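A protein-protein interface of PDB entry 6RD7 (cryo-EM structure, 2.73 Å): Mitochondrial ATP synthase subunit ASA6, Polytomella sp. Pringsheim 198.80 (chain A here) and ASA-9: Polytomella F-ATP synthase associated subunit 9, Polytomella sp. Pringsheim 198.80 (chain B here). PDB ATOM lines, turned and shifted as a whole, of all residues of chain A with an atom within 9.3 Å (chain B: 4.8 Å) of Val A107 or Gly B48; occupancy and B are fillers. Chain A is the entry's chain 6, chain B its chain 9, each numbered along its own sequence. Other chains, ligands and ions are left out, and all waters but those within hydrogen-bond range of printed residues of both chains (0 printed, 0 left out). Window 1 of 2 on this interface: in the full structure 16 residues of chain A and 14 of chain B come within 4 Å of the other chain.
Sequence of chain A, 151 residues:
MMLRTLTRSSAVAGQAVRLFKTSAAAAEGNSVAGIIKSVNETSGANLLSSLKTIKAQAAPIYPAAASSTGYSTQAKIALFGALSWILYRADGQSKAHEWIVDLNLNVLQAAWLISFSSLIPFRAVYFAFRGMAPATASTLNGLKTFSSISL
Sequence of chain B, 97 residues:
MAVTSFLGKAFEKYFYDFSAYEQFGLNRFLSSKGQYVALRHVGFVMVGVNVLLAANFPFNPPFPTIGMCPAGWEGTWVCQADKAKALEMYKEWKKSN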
ATOM      1  N   GLN A  93       6.294  36.573 -13.066  1.00  0.00           N
ATOM      2  CA  GLN A  93       6.174  35.222 -13.604  1.00  0.00           C
ATOM      3  C   GLN A  93       5.539  34.286 -12.592  1.00  0.00           C
ATOM      4  O   GLN A  93       4.816  33.357 -12.962  1.00  0.00           O
ATOM      5  CB  GLN A  93       7.547  34.690 -14.005  1.00  0.00           C
ATOM      6  CG  GLN A  93       7.988  35.056 -15.399  1.00  0.00           C
ATOM      7  CD  GLN A  93       9.347  34.490 -15.725  1.00  0.00           C
ATOM      8  OE1 GLN A  93      10.063  34.023 -14.844  1.00  0.00           O
ATOM      9  NE2 GLN A  93       9.713  34.531 -16.997  1.00  0.00           N
ATOM     10  N   ILE A 100       4.616  27.878 -12.830  1.00  0.00           N
ATOM     11  CA  ILE A 100       5.689  26.900 -12.747  1.00  0.00           C
ATOM     12  C   ILE A 100       6.240  26.605 -14.134  1.00  0.00           C
ATOM     13  O   ILE A 100       7.444  26.371 -14.287  1.00  0.00           O
ATOM     14  CB  ILE A 100       5.165  25.654 -11.995  1.00  0.00           C
ATOM     15  CG1 ILE A 100       6.260  24.610 -11.791  1.00  0.00           C
ATOM     16  CG2 ILE A 100       3.939  25.060 -12.663  1.00  0.00           C
ATOM     17  CD1 ILE A 100       7.182  24.910 -10.639  1.00  0.00           C
ATOM     18  N   VAL A 101       5.393  26.706 -15.156  1.00  0.00           N
ATOM     19  CA  VAL A 101       5.810  26.603 -16.547  1.00  0.00           C
ATOM     20  C   VAL A 101       6.803  27.705 -16.904  1.00  0.00           C
ATOM     21  O   VAL A 101       7.854  27.434 -17.491  1.00  0.00           O
ATOM     22  CB  VAL A 101       4.553  26.629 -17.434  1.00  0.00           C
ATOM     23  CG1 VAL A 101       4.887  26.926 -18.871  1.00  0.00           C
ATOM     24  CG2 VAL A 101       3.820  25.307 -17.311  1.00  0.00           C
ATOM     25  N   ASP A 102       6.521  28.945 -16.493  1.00  0.00           N
ATOM     26  CA  ASP A 102       7.441  30.057 -16.719  1.00  0.00           C
ATOM     27  C   ASP A 102       8.740  29.902 -15.935  1.00  0.00           C
ATOM     28  O   ASP A 102       9.828  30.185 -16.465  1.00  0.00           O
ATOM     29  CB  ASP A 102       6.760  31.367 -16.335  1.00  0.00           C
ATOM     30  CG  ASP A 102       5.470  31.595 -17.090  1.00  0.00           C
ATOM     31  OD1 ASP A 102       5.037  30.684 -17.820  1.00  0.00           O
ATOM     32  OD2 ASP A 102       4.883  32.687 -16.954  1.00  0.00           O
ATOM     33  N   LEU A 103       8.647  29.452 -14.682  1.00  0.00           N
ATOM     34  CA  LEU A 103       9.839  29.282 -13.863  1.00  0.00           C
ATOM     35  C   LEU A 103      10.744  28.173 -14.378  1.00  0.00           C
ATOM     36  O   LEU A 103      11.958  28.226 -14.161  1.00  0.00           O
ATOM     37  CB  LEU A 103       9.448  29.008 -12.413  1.00  0.00           C
ATOM     38  CG  LEU A 103       8.755  30.151 -11.674  1.00  0.00           C
ATOM     39  CD1 LEU A 103       8.521  29.753 -10.238  1.00  0.00           C
ATOM     40  CD2 LEU A 103       9.560  31.434 -11.751  1.00  0.00           C
ATOM     41  N   ASN A 104      10.193  27.171 -15.060  1.00  0.00           N
ATOM     42  CA  ASN A 104      11.054  26.193 -15.712  1.00  0.00           C
ATOM     43  C   ASN A 104      11.478  26.603 -17.116  1.00  0.00           C
ATOM     44  O   ASN A 104      12.491  26.094 -17.613  1.00  0.00           O
ATOM     45  CB  ASN A 104      10.391  24.818 -15.736  1.00  0.00           C
ATOM     46  CG  ASN A 104      10.232  24.244 -14.355  1.00  0.00           C
ATOM     47  OD1 ASN A 104       9.147  24.220 -13.792  1.00  0.00           O
ATOM     48  ND2 ASN A 104      11.339  23.826 -13.773  1.00  0.00           N
ATOM     49  N   LEU A 105      10.760  27.529 -17.755  1.00  0.00           N
ATOM     50  CA  LEU A 105      11.287  28.154 -18.964  1.00  0.00           C
ATOM     51  C   LEU A 105      12.556  28.943 -18.689  1.00  0.00           C
ATOM     52  O   LEU A 105      13.455  28.982 -19.541  1.00  0.00           O
ATOM     53  CB  LEU A 105      10.262  29.090 -19.588  1.00  0.00           C
ATOM     54  CG  LEU A 105       9.076  28.511 -20.338  1.00  0.00           C
ATOM     55  CD1 LEU A 105       8.511  29.599 -21.194  1.00  0.00           C
ATOM     56  CD2 LEU A 105       9.491  27.336 -21.171  1.00  0.00           C
ATOM     57  N   ASN A 106      12.630  29.581 -17.516  1.00  0.00           N
ATOM     58  CA  ASN A 106      13.861  30.261 -17.118  1.00  0.00           C
ATOM     59  C   ASN A 106      15.030  29.284 -17.008  1.00  0.00           C
ATOM     60  O   ASN A 106      16.154  29.601 -17.420  1.00  0.00           O
ATOM     61  CB  ASN A 106      13.653  30.994 -15.797  1.00  0.00           C
ATOM     62  CG  ASN A 106      12.476  31.931 -15.837  1.00  0.00           C
ATOM     63  OD1 ASN A 106      12.093  32.419 -16.896  1.00  0.00           O
ATOM     64  ND2 ASN A 106      11.887  32.185 -14.681  1.00  0.00           N
ATOM     65  N   VAL A 107      14.772  28.080 -16.493  1.00  0.00           N
ATOM     66  CA  VAL A 107      15.796  27.040 -16.415  1.00  0.00           C
ATOM     67  C   VAL A 107      16.197  26.578 -17.810  1.00  0.00           C
ATOM     68  O   VAL A 107      17.384  26.369 -18.094  1.00  0.00           O
ATOM     69  CB  VAL A 107      15.285  25.870 -15.552  1.00  0.00           C
ATOM     70  CG1 VAL A 107      16.292  24.739 -15.502  1.00  0.00           C
ATOM     71  CG2 VAL A 107      14.961  26.350 -14.156  1.00  0.00           C
ATOM     72  N   LEU A 108      15.213  26.443 -18.705  1.00  0.00           N
ATOM     73  CA  LEU A 108      15.483  26.005 -20.073  1.00  0.00           C
ATOM     74  C   LEU A 108      16.330  27.013 -20.841  1.00  0.00           C
ATOM     75  O   LEU A 108      17.136  26.634 -21.695  1.00  0.00           O
ATOM     76  CB  LEU A 108      14.169  25.770 -20.809  1.00  0.00           C
ATOM     77  CG  LEU A 108      13.572  24.375 -20.744  1.00  0.00           C
ATOM     78  CD1 LEU A 108      12.213  24.405 -21.397  1.00  0.00           C
ATOM     79  CD2 LEU A 108      14.484  23.396 -21.441  1.00  0.00           C
ATOM     80  N   GLN A 109      16.158  28.303 -20.554  1.00  0.00           N
ATOM     81  CA  GLN A 109      16.953  29.316 -21.242  1.00  0.00           C
ATOM     82  C   GLN A 109      18.342  29.464 -20.620  1.00  0.00           C
ATOM     83  O   GLN A 109      19.341  29.648 -21.339  1.00  0.00           O
ATOM     84  CB  GLN A 109      16.198  30.640 -21.239  1.00  0.00           C
ATOM     85  CG  GLN A 109      14.949  30.602 -22.099  1.00  0.00           C
ATOM     86  CD  GLN A 109      13.913  31.612 -21.676  1.00  0.00           C
ATOM     87  OE1 GLN A 109      13.949  32.125 -20.565  1.00  0.00           O
ATOM     88  NE2 GLN A 109      12.972  31.899 -22.564  1.00  0.00           N
ATOM     89  N   ALA A 110      18.432  29.372 -19.288  1.00  0.00           N
ATOM     90  CA  ALA A 110      19.729  29.417 -18.624  1.00  0.00           C
ATOM     91  C   ALA A 110      20.598  28.218 -18.971  1.00  0.00           C
ATOM     92  O   ALA A 110      21.828  28.350 -19.000  1.00  0.00           O
ATOM     93  CB  ALA A 110      19.541  29.502 -17.112  1.00  0.00           C
ATOM     94  N   ALA A 111      19.981  27.070 -19.264  1.00  0.00           N
ATOM     95  CA  ALA A 111      20.726  25.907 -19.731  1.00  0.00           C
ATOM     96  C   ALA A 111      21.432  26.173 -21.049  1.00  0.00           C
ATOM     97  O   ALA A 111      22.593  25.788 -21.213  1.00  0.00           O
ATOM     98  CB  ALA A 111      19.790  24.717 -19.886  1.00  0.00           C
ATOM     99  N   TRP A 112      20.769  26.838 -21.990  1.00  0.00           N
ATOM    100  CA  TRP A 112      21.419  27.129 -23.257  1.00  0.00           C
ATOM    101  C   TRP A 112      22.433  28.249 -23.148  1.00  0.00           C
ATOM    102  O   TRP A 112      23.402  28.254 -23.910  1.00  0.00           O
ATOM    103  CB  TRP A 112      20.394  27.466 -24.334  1.00  0.00           C
ATOM    104  CG  TRP A 112      20.057  26.294 -25.181  1.00  0.00           C
ATOM    105  CD1 TRP A 112      18.875  25.636 -25.208  1.00  0.00           C
ATOM    106  CD2 TRP A 112      20.912  25.609 -26.112  1.00  0.00           C
ATOM    107  NE1 TRP A 112      18.920  24.598 -26.099  1.00  0.00           N
ATOM    108  CE2 TRP A 112      20.163  24.560 -26.667  1.00  0.00           C
ATOM    109  CE3 TRP A 112      22.233  25.784 -26.523  1.00  0.00           C
ATOM    110  CZ2 TRP A 112      20.684  23.693 -27.613  1.00  0.00           C
ATOM    111  CZ3 TRP A 112      22.756  24.933 -27.462  1.00  0.00           C
ATOM    112  CH2 TRP A 112      21.982  23.892 -28.001  1.00  0.00           C
ATOM    113  N   LEU A 113      22.249  29.182 -22.208  1.00  0.00           N
ATOM    114  CA  LEU A 113      23.319  30.141 -21.918  1.00  0.00           C
ATOM    115  C   LEU A 113      24.574  29.436 -21.405  1.00  0.00           C
ATOM    116  O   LEU A 113      25.698  29.726 -21.849  1.00  0.00           O
ATOM    117  CB  LEU A 113      22.837  31.172 -20.902  1.00  0.00           C
ATOM    118  CG  LEU A 113      22.380  32.537 -21.407  1.00  0.00           C
ATOM    119  CD1 LEU A 113      21.121  32.419 -22.222  1.00  0.00           C
ATOM    120  CD2 LEU A 113      22.160  33.462 -20.232  1.00  0.00           C
ATOM    121  N   ILE A 114      24.389  28.475 -20.496  1.00  0.00           N
ATOM    122  CA  ILE A 114      25.502  27.698 -19.958  1.00  0.00           C
ATOM    123  C   ILE A 114      26.161  26.859 -21.053  1.00  0.00           C
ATOM    124  O   ILE A 114      27.392  26.756 -21.117  1.00  0.00           O
ATOM    125  CB  ILE A 114      24.997  26.845 -18.779  1.00  0.00           C
ATOM    126  CG1 ILE A 114      24.760  27.733 -17.558  1.00  0.00           C
ATOM    127  CG2 ILE A 114      25.962  25.744 -18.416  1.00  0.00           C
ATOM    128  CD1 ILE A 114      23.955  27.067 -16.479  1.00  0.00           C
ATOM    129  N   SER A 115      25.362  26.299 -21.963  1.00  0.00           N
ATOM    130  CA  SER A 115      25.926  25.511 -23.058  1.00  0.00           C
ATOM    131  C   SER A 115      26.632  26.380 -24.094  1.00  0.00           C
ATOM    132  O   SER A 115      27.575  25.920 -24.742  1.00  0.00           O
ATOM    133  CB  SER A 115      24.835  24.688 -23.730  1.00  0.00           C
ATOM    134  OG  SER A 115      24.305  23.727 -22.835  1.00  0.00           O
ATOM    135  N   PHE B  44      21.131  19.512 -16.314  1.00  0.00           N
ATOM    136  CA  PHE B  44      20.793  20.770 -15.657  1.00  0.00           C
ATOM    137  C   PHE B  44      19.309  21.069 -15.791  1.00  0.00           C
ATOM    138  O   PHE B  44      18.681  21.551 -14.840  1.00  0.00           O
ATOM    139  CB  PHE B  44      21.633  21.906 -16.248  1.00  0.00           C
ATOM    140  CG  PHE B  44      21.298  23.269 -15.710  1.00  0.00           C
ATOM    141  CD1 PHE B  44      21.797  23.689 -14.492  1.00  0.00           C
ATOM    142  CD2 PHE B  44      20.506  24.140 -16.438  1.00  0.00           C
ATOM    143  CE1 PHE B  44      21.494  24.943 -14.006  1.00  0.00           C
ATOM    144  CE2 PHE B  44      20.199  25.387 -15.957  1.00  0.00           C
ATOM    145  CZ  PHE B  44      20.694  25.791 -14.743  1.00  0.00           C
ATOM    146  N   VAL B  45      18.732  20.773 -16.962  1.00  0.00           N
ATOM    147  CA  VAL B  45      17.295  20.972 -17.166  1.00  0.00           C
ATOM    148  C   VAL B  45      16.493  20.059 -16.244  1.00  0.00           C
ATOM    149  O   VAL B  45      15.524  20.491 -15.606  1.00  0.00           O
ATOM    150  CB  VAL B  45      16.923  20.751 -18.644  1.00  0.00           C
ATOM    151  CG1 VAL B  45      15.422  20.787 -18.835  1.00  0.00           C
ATOM    152  CG2 VAL B  45      17.559  21.801 -19.507  1.00  0.00           C
ATOM    153  N   MET B  46      16.918  18.797 -16.121  1.00  0.00           N
ATOM    154  CA  MET B  46      16.212  17.852 -15.262  1.00  0.00           C
ATOM    155  C   MET B  46      16.347  18.201 -13.786  1.00  0.00           C
ATOM    156  O   MET B  46      15.356  18.133 -13.050  1.00  0.00           O
ATOM    157  CB  MET B  46      16.724  16.437 -15.508  1.00  0.00           C
ATOM    158  CG  MET B  46      16.161  15.790 -16.748  1.00  0.00           C
ATOM    159  SD  MET B  46      16.536  14.033 -16.809  1.00  0.00           S
ATOM    160  CE  MET B  46      18.311  14.074 -16.594  1.00  0.00           C
ATOM    161  N   VAL B  47      17.549  18.583 -13.344  1.00  0.00           N
ATOM    162  CA  VAL B  47      17.764  19.006 -11.964  1.00  0.00           C
ATOM    163  C   VAL B  47      16.952  20.258 -11.647  1.00  0.00           C
ATOM    164  O   VAL B  47      16.352  20.362 -10.570  1.00  0.00           O
ATOM    165  CB  VAL B  47      19.273  19.197 -11.706  1.00  0.00           C
ATOM    166  CG1 VAL B  47      19.533  19.951 -10.429  1.00  0.00           C
ATOM    167  CG2 VAL B  47      19.951  17.842 -11.591  1.00  0.00           C
ATOM    168  N   GLY B  48      16.857  21.192 -12.598  1.00  0.00           N
ATOM    169  CA  GLY B  48      16.064  22.390 -12.370  1.00  0.00           C
ATOM    170  C   GLY B  48      14.575  22.110 -12.296  1.00  0.00           C
ATOM    171  O   GLY B  48      13.880  22.652 -11.433  1.00  0.00           O
ATOM    172  N   VAL B  49      14.071  21.239 -13.176  1.00  0.00           N
ATOM    173  CA  VAL B  49      12.664  20.846 -13.134  1.00  0.00           C
ATOM    174  C   VAL B  49      12.337  20.130 -11.830  1.00  0.00           C
ATOM    175  O   VAL B  49      11.322  20.430 -11.181  1.00  0.00           O
ATOM    176  CB  VAL B  49      12.337  19.993 -14.374  1.00  0.00           C
ATOM    177  CG1 VAL B  49      11.076  19.168 -14.187  1.00  0.00           C
ATOM    178  CG2 VAL B  49      12.195  20.881 -15.594  1.00  0.00           C
ATOM    179  N   ASN B  50      13.223  19.243 -11.380  1.00  0.00           N
ATOM    180  CA  ASN B  50      12.977  18.510 -10.150  1.00  0.00           C
ATOM    181  C   ASN B  50      13.067  19.390  -8.908  1.00  0.00           C
ATOM    182  O   ASN B  50      12.261  19.214  -7.995  1.00  0.00           O
ATOM    183  CB  ASN B  50      13.940  17.337 -10.041  1.00  0.00           C
ATOM    184  CG  ASN B  50      13.737  16.325 -11.141  1.00  0.00           C
ATOM    185  OD1 ASN B  50      12.678  16.276 -11.765  1.00  0.00           O
ATOM    186  ND2 ASN B  50      14.750  15.506 -11.386  1.00  0.00           N
ATOM    187  N   VAL B  51      13.983  20.364  -8.853  1.00  0.00           N
ATOM    188  CA  VAL B  51      14.041  21.193  -7.650  1.00  0.00           C
ATOM    189  C   VAL B  51      12.941  22.252  -7.664  1.00  0.00           C
ATOM    190  O   VAL B  51      12.472  22.680  -6.603  1.00  0.00           O
ATOM    191  CB  VAL B  51      15.439  21.816  -7.444  1.00  0.00           C
ATOM    192  CG1 VAL B  51      16.509  20.728  -7.326  1.00  0.00           C
ATOM    193  CG2 VAL B  51      15.783  22.837  -8.513  1.00  0.00           C
ATOM    194  N   LEU B  52      12.480  22.669  -8.849  1.00  0.00           N
ATOM    195  CA  LEU B  52      11.343  23.586  -8.906  1.00  0.00           C
ATOM    196  C   LEU B  52      10.045  22.871  -8.551  1.00  0.00           C
ATOM    197  O   LEU B  52       9.098  23.491  -8.057  1.00  0.00           O
ATOM    198  CB  LEU B  52      11.247  24.241 -10.287  1.00  0.00           C
ATOM    199  CG  LEU B  52      11.887  25.608 -10.576  1.00  0.00           C
ATOM    200  CD1 LEU B  52      11.190  26.677  -9.773  1.00  0.00           C
ATOM    201  CD2 LEU B  52      13.366  25.639 -10.270  1.00  0.00           C
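The side-chain amide oxygen (OD1) of Asn A104 lies close to the backbone carbonyl oxygen (O) of Ile A100, 2.8 Å away. The backbone carbonyl oxygen of Ala A111 is in hydrogen-bond range of the side-chain hydroxyl of Ser A115 (3.1 Å).
Ile A100 touches Leu B52 (CD1 to O, 3.5 Å). CB of Leu A103 touches CD1 of Leu B52, 3.9 Å away. ND2 of Asn A104 touches O of Gly B48 (3.6 Å). Asn A104 touches Leu B52. O of Val A107 touches CE2 of Phe B44, 3.7 Å away. Val A107 touches Gly B48. Leu A108 touches Val B45. Ala A111 touches Phe B44. Val B45 touches Ala A111 (CG2 to CB, 3.7 Å). Ile A114 touches Phe B44 (CD1 to CZ, 3.9 Å).
Leu A105 touches none of the printed residues of chain B. Val A107 touches just these residues of chain B: Phe B44 (3.7 Å) and Gly B48 (3.9 Å). Of the printed residues of chain B, Leu A108 touches Val B45 (3.8 Å). Ala A110 touches none of the printed residues of chain B. Of the printed residues of chain B, Ala A111 touches Phe B44 (3.6 Å) and Val B45 (3.7 Å). Of the printed residues of chain B, Ile A114 touches Phe B44. Val B45 touches just these residues of chain A: Leu A108 and Ala A111. Of chain A, only Asn A104 (3.6 Å) and Val A107 (3.9 Å) come within 4 Å of Gly B48. Of the printed residues of chain A, Val B49 touches Asn A104. No residue of chain A comes within 4 Å of Val B51. The nearest residue of chain A that does not touch Gly B48 is Leu A103 (6.5 Å).
Printed residues of chain B that touch a printed residue of chain A: Phe B44, Val B45, Gly B48, Val B49 and Leu B52. Hydrophobic or aromatic side chains of chain B that line the printed part of chain A: Phe B44, Val B45, Val B49 and Leu B52. Among the printed residues, no Asp or Glu carboxylate lies within 4 Å of a Lys or Arg side-chain nitrogen of the other chain.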
